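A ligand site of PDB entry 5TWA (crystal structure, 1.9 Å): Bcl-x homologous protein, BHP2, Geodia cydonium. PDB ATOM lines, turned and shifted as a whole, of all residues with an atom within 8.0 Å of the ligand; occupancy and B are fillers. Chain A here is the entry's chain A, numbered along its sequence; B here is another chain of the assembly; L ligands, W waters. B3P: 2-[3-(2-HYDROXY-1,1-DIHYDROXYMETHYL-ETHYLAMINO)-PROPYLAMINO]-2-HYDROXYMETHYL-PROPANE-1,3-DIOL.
OH of Tyr 177 is in hydrogen-bond range of N of Gly 121 (3.4 Å).
OH of Tyr 177 lies within hydrogen-bond range of OD1 of Asp 20 of chain B (2.6 Å).
The backbone carbonyl oxygen of Glu 168 is in hydrogen-bond range of an oxygen (O4) of the ligand (2.6 Å).
OE1 of Glu 168 is in salt-bridge range of N1 of the ligand, at 3.0 Å.
An oxygen (O5) of the ligand is in hydrogen-bond range of the side-chain amide nitrogen (ND2) of Asn 169.
The side-chain hydroxyl (OH) of Tyr 24 of chain B sits at hydrogen-bond distance from an oxygen (O3) of the ligand (2.9 Å).
O4 of the ligand sits close to O of Gly 173 (3.4 Å).
The indole nitrogen (NE1) of Trp 120 sits at hydrogen-bond distance from an oxygen (O4) of the ligand (3.0 Å).
Residues that only touch the ligand: Tyr 177 (3.8 Å) and Phe 23 of chain B (3.6 Å).
Hydrophobic or aromatic side chains within 4 Å of the ligand: Trp 120, Tyr 177, Phe 23 of chain B and Tyr 24 of chain B.
The nearest printed residue that does not touch the ligand is Phe 174 (4.2 Å).
Water W1 lies within hydrogen-bond range of OE2 of Glu 168 (2.7 Å) and N2 of the ligand (2.9 Å).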
ATOM      1  N   HIS A 119      -4.744  -4.973   1.762  1.00  0.00           N
ATOM      2  CA  HIS A 119      -4.699  -3.702   2.482  1.00  0.00           C
ATOM      3  C   HIS A 119      -5.963  -2.929   2.159  1.00  0.00           C
ATOM      4  O   HIS A 119      -6.777  -3.357   1.334  1.00  0.00           O
ATOM      5  CB  HIS A 119      -3.422  -2.909   2.156  1.00  0.00           C
ATOM      6  CG  HIS A 119      -3.224  -2.593   0.708  1.00  0.00           C
ATOM      7  ND1 HIS A 119      -4.078  -1.777  -0.007  1.00  0.00           N
ATOM      8  CD2 HIS A 119      -2.233  -2.930  -0.144  1.00  0.00           C
ATOM      9  CE1 HIS A 119      -3.642  -1.657  -1.242  1.00  0.00           C
ATOM     10  NE2 HIS A 119      -2.523  -2.348  -1.355  1.00  0.00           N
ATOM     11  N   TRP A 120      -6.165  -1.797   2.855  1.00  0.00           N
ATOM     12  CA  TRP A 120      -7.450  -1.109   2.739  1.00  0.00           C
ATOM     13  C   TRP A 120      -7.717  -0.650   1.311  1.00  0.00           C
ATOM     14  O   TRP A 120      -8.877  -0.637   0.861  1.00  0.00           O
ATOM     15  CB  TRP A 120      -7.506   0.086   3.701  1.00  0.00           C
ATOM     16  CG  TRP A 120      -7.921  -0.183   5.124  1.00  0.00           C
ATOM     17  CD1 TRP A 120      -7.236   0.208   6.253  1.00  0.00           C
ATOM     18  CD2 TRP A 120      -9.124  -0.828   5.591  1.00  0.00           C
ATOM     19  NE1 TRP A 120      -7.929  -0.170   7.373  1.00  0.00           N
ATOM     20  CE2 TRP A 120      -9.081  -0.809   6.999  1.00  0.00           C
ATOM     21  CE3 TRP A 120     -10.222  -1.426   4.957  1.00  0.00           C
ATOM     22  CZ2 TRP A 120     -10.086  -1.370   7.791  1.00  0.00           C
ATOM     23  CZ3 TRP A 120     -11.222  -1.974   5.745  1.00  0.00           C
ATOM     24  CH2 TRP A 120     -11.145  -1.949   7.138  1.00  0.00           C
ATOM     25  N   GLY A 121      -6.674  -0.258   0.586  1.00  0.00           N
ATOM     26  CA  GLY A 121      -6.876   0.183  -0.790  1.00  0.00           C
ATOM     27  C   GLY A 121      -7.485  -0.890  -1.672  1.00  0.00           C
ATOM     28  O   GLY A 121      -8.405  -0.629  -2.450  1.00  0.00           O
ATOM     29  N   PHE A 164      -7.782  -9.203   8.465  1.00  0.00           N
ATOM     30  CA  PHE A 164      -7.248  -7.886   8.139  1.00  0.00           C
ATOM     31  C   PHE A 164      -8.075  -6.780   8.766  1.00  0.00           C
ATOM     32  O   PHE A 164      -7.543  -5.854   9.380  1.00  0.00           O
ATOM     33  CB  PHE A 164      -7.181  -7.689   6.622  1.00  0.00           C
ATOM     34  CG  PHE A 164      -6.881  -6.273   6.238  1.00  0.00           C
ATOM     35  CD1 PHE A 164      -5.600  -5.784   6.314  1.00  0.00           C
ATOM     36  CD2 PHE A 164      -7.898  -5.407   5.838  1.00  0.00           C
ATOM     37  CE1 PHE A 164      -5.309  -4.472   5.991  1.00  0.00           C
ATOM     38  CE2 PHE A 164      -7.615  -4.095   5.503  1.00  0.00           C
ATOM     39  CZ  PHE A 164      -6.317  -3.628   5.586  1.00  0.00           C
ATOM     40  N   ILE A 165      -9.398  -6.842   8.583  1.00  0.00           N
ATOM     41  CA  ILE A 165     -10.272  -5.776   9.071  1.00  0.00           C
ATOM     42  C   ILE A 165     -10.103  -5.587  10.576  1.00  0.00           C
ATOM     43  O   ILE A 165      -9.939  -4.466  11.066  1.00  0.00           O
ATOM     44  CB  ILE A 165     -11.744  -6.087   8.707  1.00  0.00           C
ATOM     45  CG1 ILE A 165     -11.954  -5.943   7.202  1.00  0.00           C
ATOM     46  CG2 ILE A 165     -12.691  -5.160   9.474  1.00  0.00           C
ATOM     47  CD1 ILE A 165     -13.204  -6.622   6.675  1.00  0.00           C
ATOM     48  N   GLN A 166     -10.107  -6.691  11.329  1.00  0.00           N
ATOM     49  CA  GLN A 166      -9.960  -6.573  12.783  1.00  0.00           C
ATOM     50  C   GLN A 166      -8.567  -6.104  13.170  1.00  0.00           C
ATOM     51  O   GLN A 166      -8.403  -5.339  14.125  1.00  0.00           O
ATOM     52  CB  GLN A 166     -10.278  -7.921  13.443  1.00  0.00           C
ATOM     53  CG  GLN A 166     -11.708  -8.393  13.228  1.00  0.00           C
ATOM     54  CD  GLN A 166     -12.734  -7.544  13.948  1.00  0.00           C
ATOM     55  OE1 GLN A 166     -13.030  -6.417  13.552  1.00  0.00           O
ATOM     56  NE2 GLN A 166     -13.297  -8.089  15.028  1.00  0.00           N
ATOM     57  N   ARG A 167      -7.530  -6.548  12.444  1.00  0.00           N
ATOM     58  CA  ARG A 167      -6.172  -6.101  12.717  1.00  0.00           C
ATOM     59  C   ARG A 167      -6.034  -4.588  12.568  1.00  0.00           C
ATOM     60  O   ARG A 167      -5.260  -3.937  13.293  1.00  0.00           O
ATOM     61  CB  ARG A 167      -5.198  -6.809  11.771  1.00  0.00           C
ATOM     62  CG  ARG A 167      -3.744  -6.398  11.895  1.00  0.00           C
ATOM     63  CD  ARG A 167      -2.886  -7.099  10.848  1.00  0.00           C
ATOM     64  NE  ARG A 167      -3.330  -8.481  10.618  1.00  0.00           N
ATOM     65  CZ  ARG A 167      -3.652  -8.980   9.426  1.00  0.00           C
ATOM     66  NH1 ARG A 167      -3.549  -8.232   8.335  1.00  0.00           N
ATOM     67  NH2 ARG A 167      -4.046 -10.240   9.321  1.00  0.00           N
ATOM     68  N   GLU A 168      -6.771  -3.988  11.637  1.00  0.00           N
ATOM     69  CA  GLU A 168      -6.686  -2.558  11.381  1.00  0.00           C
ATOM     70  C   GLU A 168      -7.773  -1.777  12.111  1.00  0.00           C
ATOM     71  O   GLU A 168      -8.161  -0.688  11.651  1.00  0.00           O
ATOM     72  CB  GLU A 168      -6.715  -2.289   9.876  1.00  0.00           C
ATOM     73  CG  GLU A 168      -5.553  -2.969   9.108  1.00  0.00           C
ATOM     74  CD  GLU A 168      -4.172  -2.551   9.624  1.00  0.00           C
ATOM     75  OE1 GLU A 168      -4.045  -1.445  10.173  1.00  0.00           O
ATOM     76  OE2 GLU A 168      -3.204  -3.350   9.481  1.00  0.00           O
ATOM     77  N   ASN A 169      -8.257  -2.307  13.239  1.00  0.00           N
ATOM     78  CA  ASN A 169      -9.188  -1.625  14.132  1.00  0.00           C
ATOM     79  C   ASN A 169     -10.587  -1.520  13.541  1.00  0.00           C
ATOM     80  O   ASN A 169     -11.341  -0.583  13.841  1.00  0.00           O
ATOM     81  CB  ASN A 169      -8.652  -0.247  14.546  1.00  0.00           C
ATOM     82  CG  ASN A 169      -7.585  -0.345  15.603  1.00  0.00           C
ATOM     83  OD1 ASN A 169      -7.596  -1.273  16.407  1.00  0.00           O
ATOM     84  ND2 ASN A 169      -6.657   0.611  15.613  1.00  0.00           N
ATOM     85  N   GLY A 170     -10.978  -2.489  12.712  1.00  0.00           N
ATOM     86  CA  GLY A 170     -12.351  -2.578  12.273  1.00  0.00           C
ATOM     87  C   GLY A 170     -12.776  -1.389  11.424  1.00  0.00           C
ATOM     88  O   GLY A 170     -11.967  -0.648  10.862  1.00  0.00           O
ATOM     89  N   TRP A 171     -14.106  -1.212  11.339  1.00  0.00           N
ATOM     90  CA  TRP A 171     -14.623  -0.092  10.555  1.00  0.00           C
ATOM     91  C   TRP A 171     -14.370   1.247  11.224  1.00  0.00           C
ATOM     92  O   TRP A 171     -14.365   2.277  10.541  1.00  0.00           O
ATOM     93  CB  TRP A 171     -16.114  -0.319  10.287  1.00  0.00           C
ATOM     94  CG  TRP A 171     -16.305  -1.507   9.390  1.00  0.00           C
ATOM     95  CD1 TRP A 171     -16.879  -2.696   9.722  1.00  0.00           C
ATOM     96  CD2 TRP A 171     -15.879  -1.625   8.034  1.00  0.00           C
ATOM     97  NE1 TRP A 171     -16.861  -3.550   8.637  1.00  0.00           N
ATOM     98  CE2 TRP A 171     -16.245  -2.907   7.585  1.00  0.00           C
ATOM     99  CE3 TRP A 171     -15.234  -0.765   7.134  1.00  0.00           C
ATOM    100  CZ2 TRP A 171     -15.987  -3.357   6.295  1.00  0.00           C
ATOM    101  CZ3 TRP A 171     -14.976  -1.204   5.853  1.00  0.00           C
ATOM    102  CH2 TRP A 171     -15.360  -2.502   5.434  1.00  0.00           C
ATOM    103  N   ARG A 172     -14.130   1.247  12.542  1.00  0.00           N
ATOM    104  CA  ARG A 172     -13.655   2.474  13.184  1.00  0.00           C
ATOM    105  C   ARG A 172     -12.291   2.861  12.625  1.00  0.00           C
ATOM    106  O   ARG A 172     -12.044   4.033  12.303  1.00  0.00           O
ATOM    107  CB  ARG A 172     -13.576   2.258  14.696  1.00  0.00           C
ATOM    108  CG  ARG A 172     -13.535   3.536  15.486  1.00  0.00           C
ATOM    109  CD  ARG A 172     -14.934   3.978  15.868  1.00  0.00           C
ATOM    110  NE  ARG A 172     -15.443   3.244  17.021  1.00  0.00           N
ATOM    111  CZ  ARG A 172     -16.403   3.688  17.822  1.00  0.00           C
ATOM    112  NH1 ARG A 172     -16.947   4.880  17.601  1.00  0.00           N
ATOM    113  NH2 ARG A 172     -16.809   2.971  18.852  1.00  0.00           N
ATOM    114  N   GLY A 173     -11.404   1.881  12.484  1.00  0.00           N
ATOM    115  CA  GLY A 173     -10.106   2.156  11.888  1.00  0.00           C
ATOM    116  C   GLY A 173     -10.212   2.592  10.438  1.00  0.00           C
ATOM    117  O   GLY A 173      -9.445   3.426   9.971  1.00  0.00           O
ATOM    118  N   PHE A 174     -11.163   2.016   9.703  1.00  0.00           N
ATOM    119  CA  PHE A 174     -11.301   2.403   8.311  1.00  0.00           C
ATOM    120  C   PHE A 174     -11.616   3.890   8.189  1.00  0.00           C
ATOM    121  O   PHE A 174     -11.117   4.567   7.276  1.00  0.00           O
ATOM    122  CB  PHE A 174     -12.383   1.608   7.596  1.00  0.00           C
ATOM    123  CG  PHE A 174     -12.645   2.111   6.215  1.00  0.00           C
ATOM    124  CD1 PHE A 174     -11.767   1.821   5.190  1.00  0.00           C
ATOM    125  CD2 PHE A 174     -13.719   2.949   5.958  1.00  0.00           C
ATOM    126  CE1 PHE A 174     -11.984   2.317   3.924  1.00  0.00           C
ATOM    127  CE2 PHE A 174     -13.942   3.439   4.688  1.00  0.00           C
ATOM    128  CZ  PHE A 174     -13.061   3.125   3.670  1.00  0.00           C
ATOM    129  N   ILE A 175     -12.451   4.411   9.090  1.00  0.00           N
ATOM    130  CA  ILE A 175     -12.837   5.826   9.028  1.00  0.00           C
ATOM    131  C   ILE A 175     -11.620   6.723   9.244  1.00  0.00           C
ATOM    132  O   ILE A 175     -11.470   7.750   8.582  1.00  0.00           O
ATOM    133  CB  ILE A 175     -13.951   6.112  10.042  1.00  0.00           C
ATOM    134  CG1 ILE A 175     -15.246   5.408   9.632  1.00  0.00           C
ATOM    135  CG2 ILE A 175     -14.155   7.621  10.212  1.00  0.00           C
ATOM    136  CD1 ILE A 175     -16.270   5.322  10.736  1.00  0.00           C
ATOM    137  N   VAL A 176     -10.751   6.352  10.189  1.00  0.00           N
ATOM    138  CA  VAL A 176      -9.488   7.076  10.389  1.00  0.00           C
ATOM    139  C   VAL A 176      -8.642   7.023   9.121  1.00  0.00           C
ATOM    140  O   VAL A 176      -8.094   8.036   8.668  1.00  0.00           O
ATOM    141  CB  VAL A 176      -8.727   6.503  11.595  1.00  0.00           C
ATOM    142  CG1 VAL A 176      -7.315   7.075  11.673  1.00  0.00           C
ATOM    143  CG2 VAL A 176      -9.501   6.752  12.876  1.00  0.00           C
ATOM    144  N   TYR A 177      -8.522   5.826   8.543  1.00  0.00           N
ATOM    145  CA  TYR A 177      -7.777   5.647   7.297  1.00  0.00           C
ATOM    146  C   TYR A 177      -8.392   6.480   6.178  1.00  0.00           C
ATOM    147  O   TYR A 177      -7.673   7.161   5.432  1.00  0.00           O
ATOM    148  CB  TYR A 177      -7.785   4.161   6.928  1.00  0.00           C
ATOM    149  CG  TYR A 177      -7.260   3.800   5.556  1.00  0.00           C
ATOM    150  CD1 TYR A 177      -5.913   3.514   5.359  1.00  0.00           C
ATOM    151  CD2 TYR A 177      -8.108   3.705   4.459  1.00  0.00           C
ATOM    152  CE1 TYR A 177      -5.432   3.180   4.118  1.00  0.00           C
ATOM    153  CE2 TYR A 177      -7.639   3.358   3.210  1.00  0.00           C
ATOM    154  CZ  TYR A 177      -6.294   3.099   3.048  1.00  0.00           C
ATOM    155  OH  TYR A 177      -5.802   2.748   1.818  1.00  0.00           O
ATOM    156  N   ALA A 178      -9.716   6.451   6.046  1.00  0.00           N
ATOM    157  CA  ALA A 178     -10.371   7.126   4.927  1.00  0.00           C
ATOM    158  C   ALA A 178     -10.304   8.640   5.075  1.00  0.00           C
ATOM    159  O   ALA A 178     -10.059   9.349   4.094  1.00  0.00           O
ATOM    160  CB  ALA A 178     -11.815   6.658   4.808  1.00  0.00           C
ATOM    161  N   THR A 180      -7.949  10.272   6.372  1.00  0.00           N
ATOM    162  CA  THR A 180      -6.599  10.610   5.919  1.00  0.00           C
ATOM    163  C   THR A 180      -6.534  10.683   4.408  1.00  0.00           C
ATOM    164  O   THR A 180      -5.915  11.594   3.850  1.00  0.00           O
ATOM    165  CB  THR A 180      -5.591   9.577   6.434  1.00  0.00           C
ATOM    166  OG1 THR A 180      -5.534   9.615   7.866  1.00  0.00           O
ATOM    167  CG2 THR A 180      -4.203   9.841   5.863  1.00  0.00           C
ATOM    168  N   ASP B  20      -3.998   3.209  -1.570  1.00  0.00           N
ATOM    169  CA  ASP B  20      -3.347   3.030  -0.278  1.00  0.00           C
ATOM    170  C   ASP B  20      -2.103   3.901  -0.138  1.00  0.00           C
ATOM    171  O   ASP B  20      -1.779   4.341   0.969  1.00  0.00           O
ATOM    172  CB  ASP B  20      -2.999   1.554  -0.076  1.00  0.00           C
ATOM    173  CG  ASP B  20      -2.738   1.193   1.378  1.00  0.00           C
ATOM    174  OD1 ASP B  20      -3.642   1.374   2.218  1.00  0.00           O
ATOM    175  OD2 ASP B  20      -1.627   0.709   1.674  1.00  0.00           O
ATOM    176  N   PHE B  23      -2.455   7.160   1.729  1.00  0.00           N
ATOM    177  CA  PHE B  23      -2.526   7.201   3.189  1.00  0.00           C
ATOM    178  C   PHE B  23      -1.179   7.603   3.789  1.00  0.00           C
ATOM    179  O   PHE B  23      -1.142   8.257   4.835  1.00  0.00           O
ATOM    180  CB  PHE B  23      -2.950   5.843   3.758  1.00  0.00           C
ATOM    181  CG  PHE B  23      -2.893   5.765   5.255  1.00  0.00           C
ATOM    182  CD1 PHE B  23      -3.917   6.290   6.028  1.00  0.00           C
ATOM    183  CD2 PHE B  23      -1.807   5.192   5.897  1.00  0.00           C
ATOM    184  CE1 PHE B  23      -3.865   6.242   7.408  1.00  0.00           C
ATOM    185  CE2 PHE B  23      -1.749   5.139   7.272  1.00  0.00           C
ATOM    186  CZ  PHE B  23      -2.780   5.652   8.025  1.00  0.00           C
ATOM    187  N   TYR B  24      -0.085   7.203   3.151  1.00  0.00           N
ATOM    188  CA  TYR B  24       1.250   7.476   3.627  1.00  0.00           C
ATOM    189  C   TYR B  24       1.806   8.786   3.098  1.00  0.00           C
ATOM    190  O   TYR B  24       2.983   9.075   3.320  1.00  0.00           O
ATOM    191  CB  TYR B  24       2.174   6.317   3.236  1.00  0.00           C
ATOM    192  CG  TYR B  24       1.723   4.991   3.797  1.00  0.00           C
ATOM    193  CD1 TYR B  24       2.142   4.577   5.051  1.00  0.00           C
ATOM    194  CD2 TYR B  24       0.868   4.159   3.075  1.00  0.00           C
ATOM    195  CE1 TYR B  24       1.722   3.363   5.578  1.00  0.00           C
ATOM    196  CE2 TYR B  24       0.456   2.940   3.597  1.00  0.00           C
ATOM    197  CZ  TYR B  24       0.878   2.556   4.848  1.00  0.00           C
ATOM    198  OH  TYR B  24       0.485   1.357   5.382  1.00  0.00           O
HETATM  199  C1  B3P L   1      -3.466   1.372   7.621  1.00  0.00           C
HETATM  200  C2  B3P L   1      -1.985   1.593   8.041  1.00  0.00           C
HETATM  201  C3  B3P L   1      -4.437   2.140   8.538  1.00  0.00           C
HETATM  202  N1  B3P L   1      -4.365   1.542   9.880  1.00  0.00           N
HETATM  203  C4  B3P L   1      -5.201   2.251  10.852  1.00  0.00           C
HETATM  204  C5  B3P L   1      -6.649   2.260  10.375  1.00  0.00           C
HETATM  205  C6  B3P L   1      -5.069   1.498  12.202  1.00  0.00           C
HETATM  206  C7  B3P L   1      -4.715   3.696  11.008  1.00  0.00           C
HETATM  207  N2  B3P L   1      -1.617   0.667   9.134  1.00  0.00           N
HETATM  208  C8  B3P L   1      -0.349   1.048   9.797  1.00  0.00           C
HETATM  209  C9  B3P L   1      -0.584   2.267  10.709  1.00  0.00           C
HETATM  210  C10 B3P L   1       0.140  -0.132  10.654  1.00  0.00           C
HETATM  211  C11 B3P L   1       0.725   1.412   8.760  1.00  0.00           C
HETATM  212  O1  B3P L   1      -1.535   1.919  11.695  1.00  0.00           O
HETATM  213  O2  B3P L   1       1.291   0.235  11.354  1.00  0.00           O
HETATM  214  O3  B3P L   1       1.066   0.260   8.048  1.00  0.00           O
HETATM  215  O4  B3P L   1      -7.069   0.964  10.041  1.00  0.00           O
HETATM  216  O5  B3P L   1      -5.898   2.072  13.184  1.00  0.00           O
HETATM  217  O6  B3P L   1      -3.438   3.728  11.575  1.00  0.00           O
HETATM  218  O   HOH W   1      -1.279  -2.000   8.068  1.00  0.00           O
HETATM  219  O   HOH W   2       1.073  -3.165   7.980  1.00  0.00           O
HETATM  220  O   HOH W   3       3.879   0.429   8.058  1.00  0.00           O
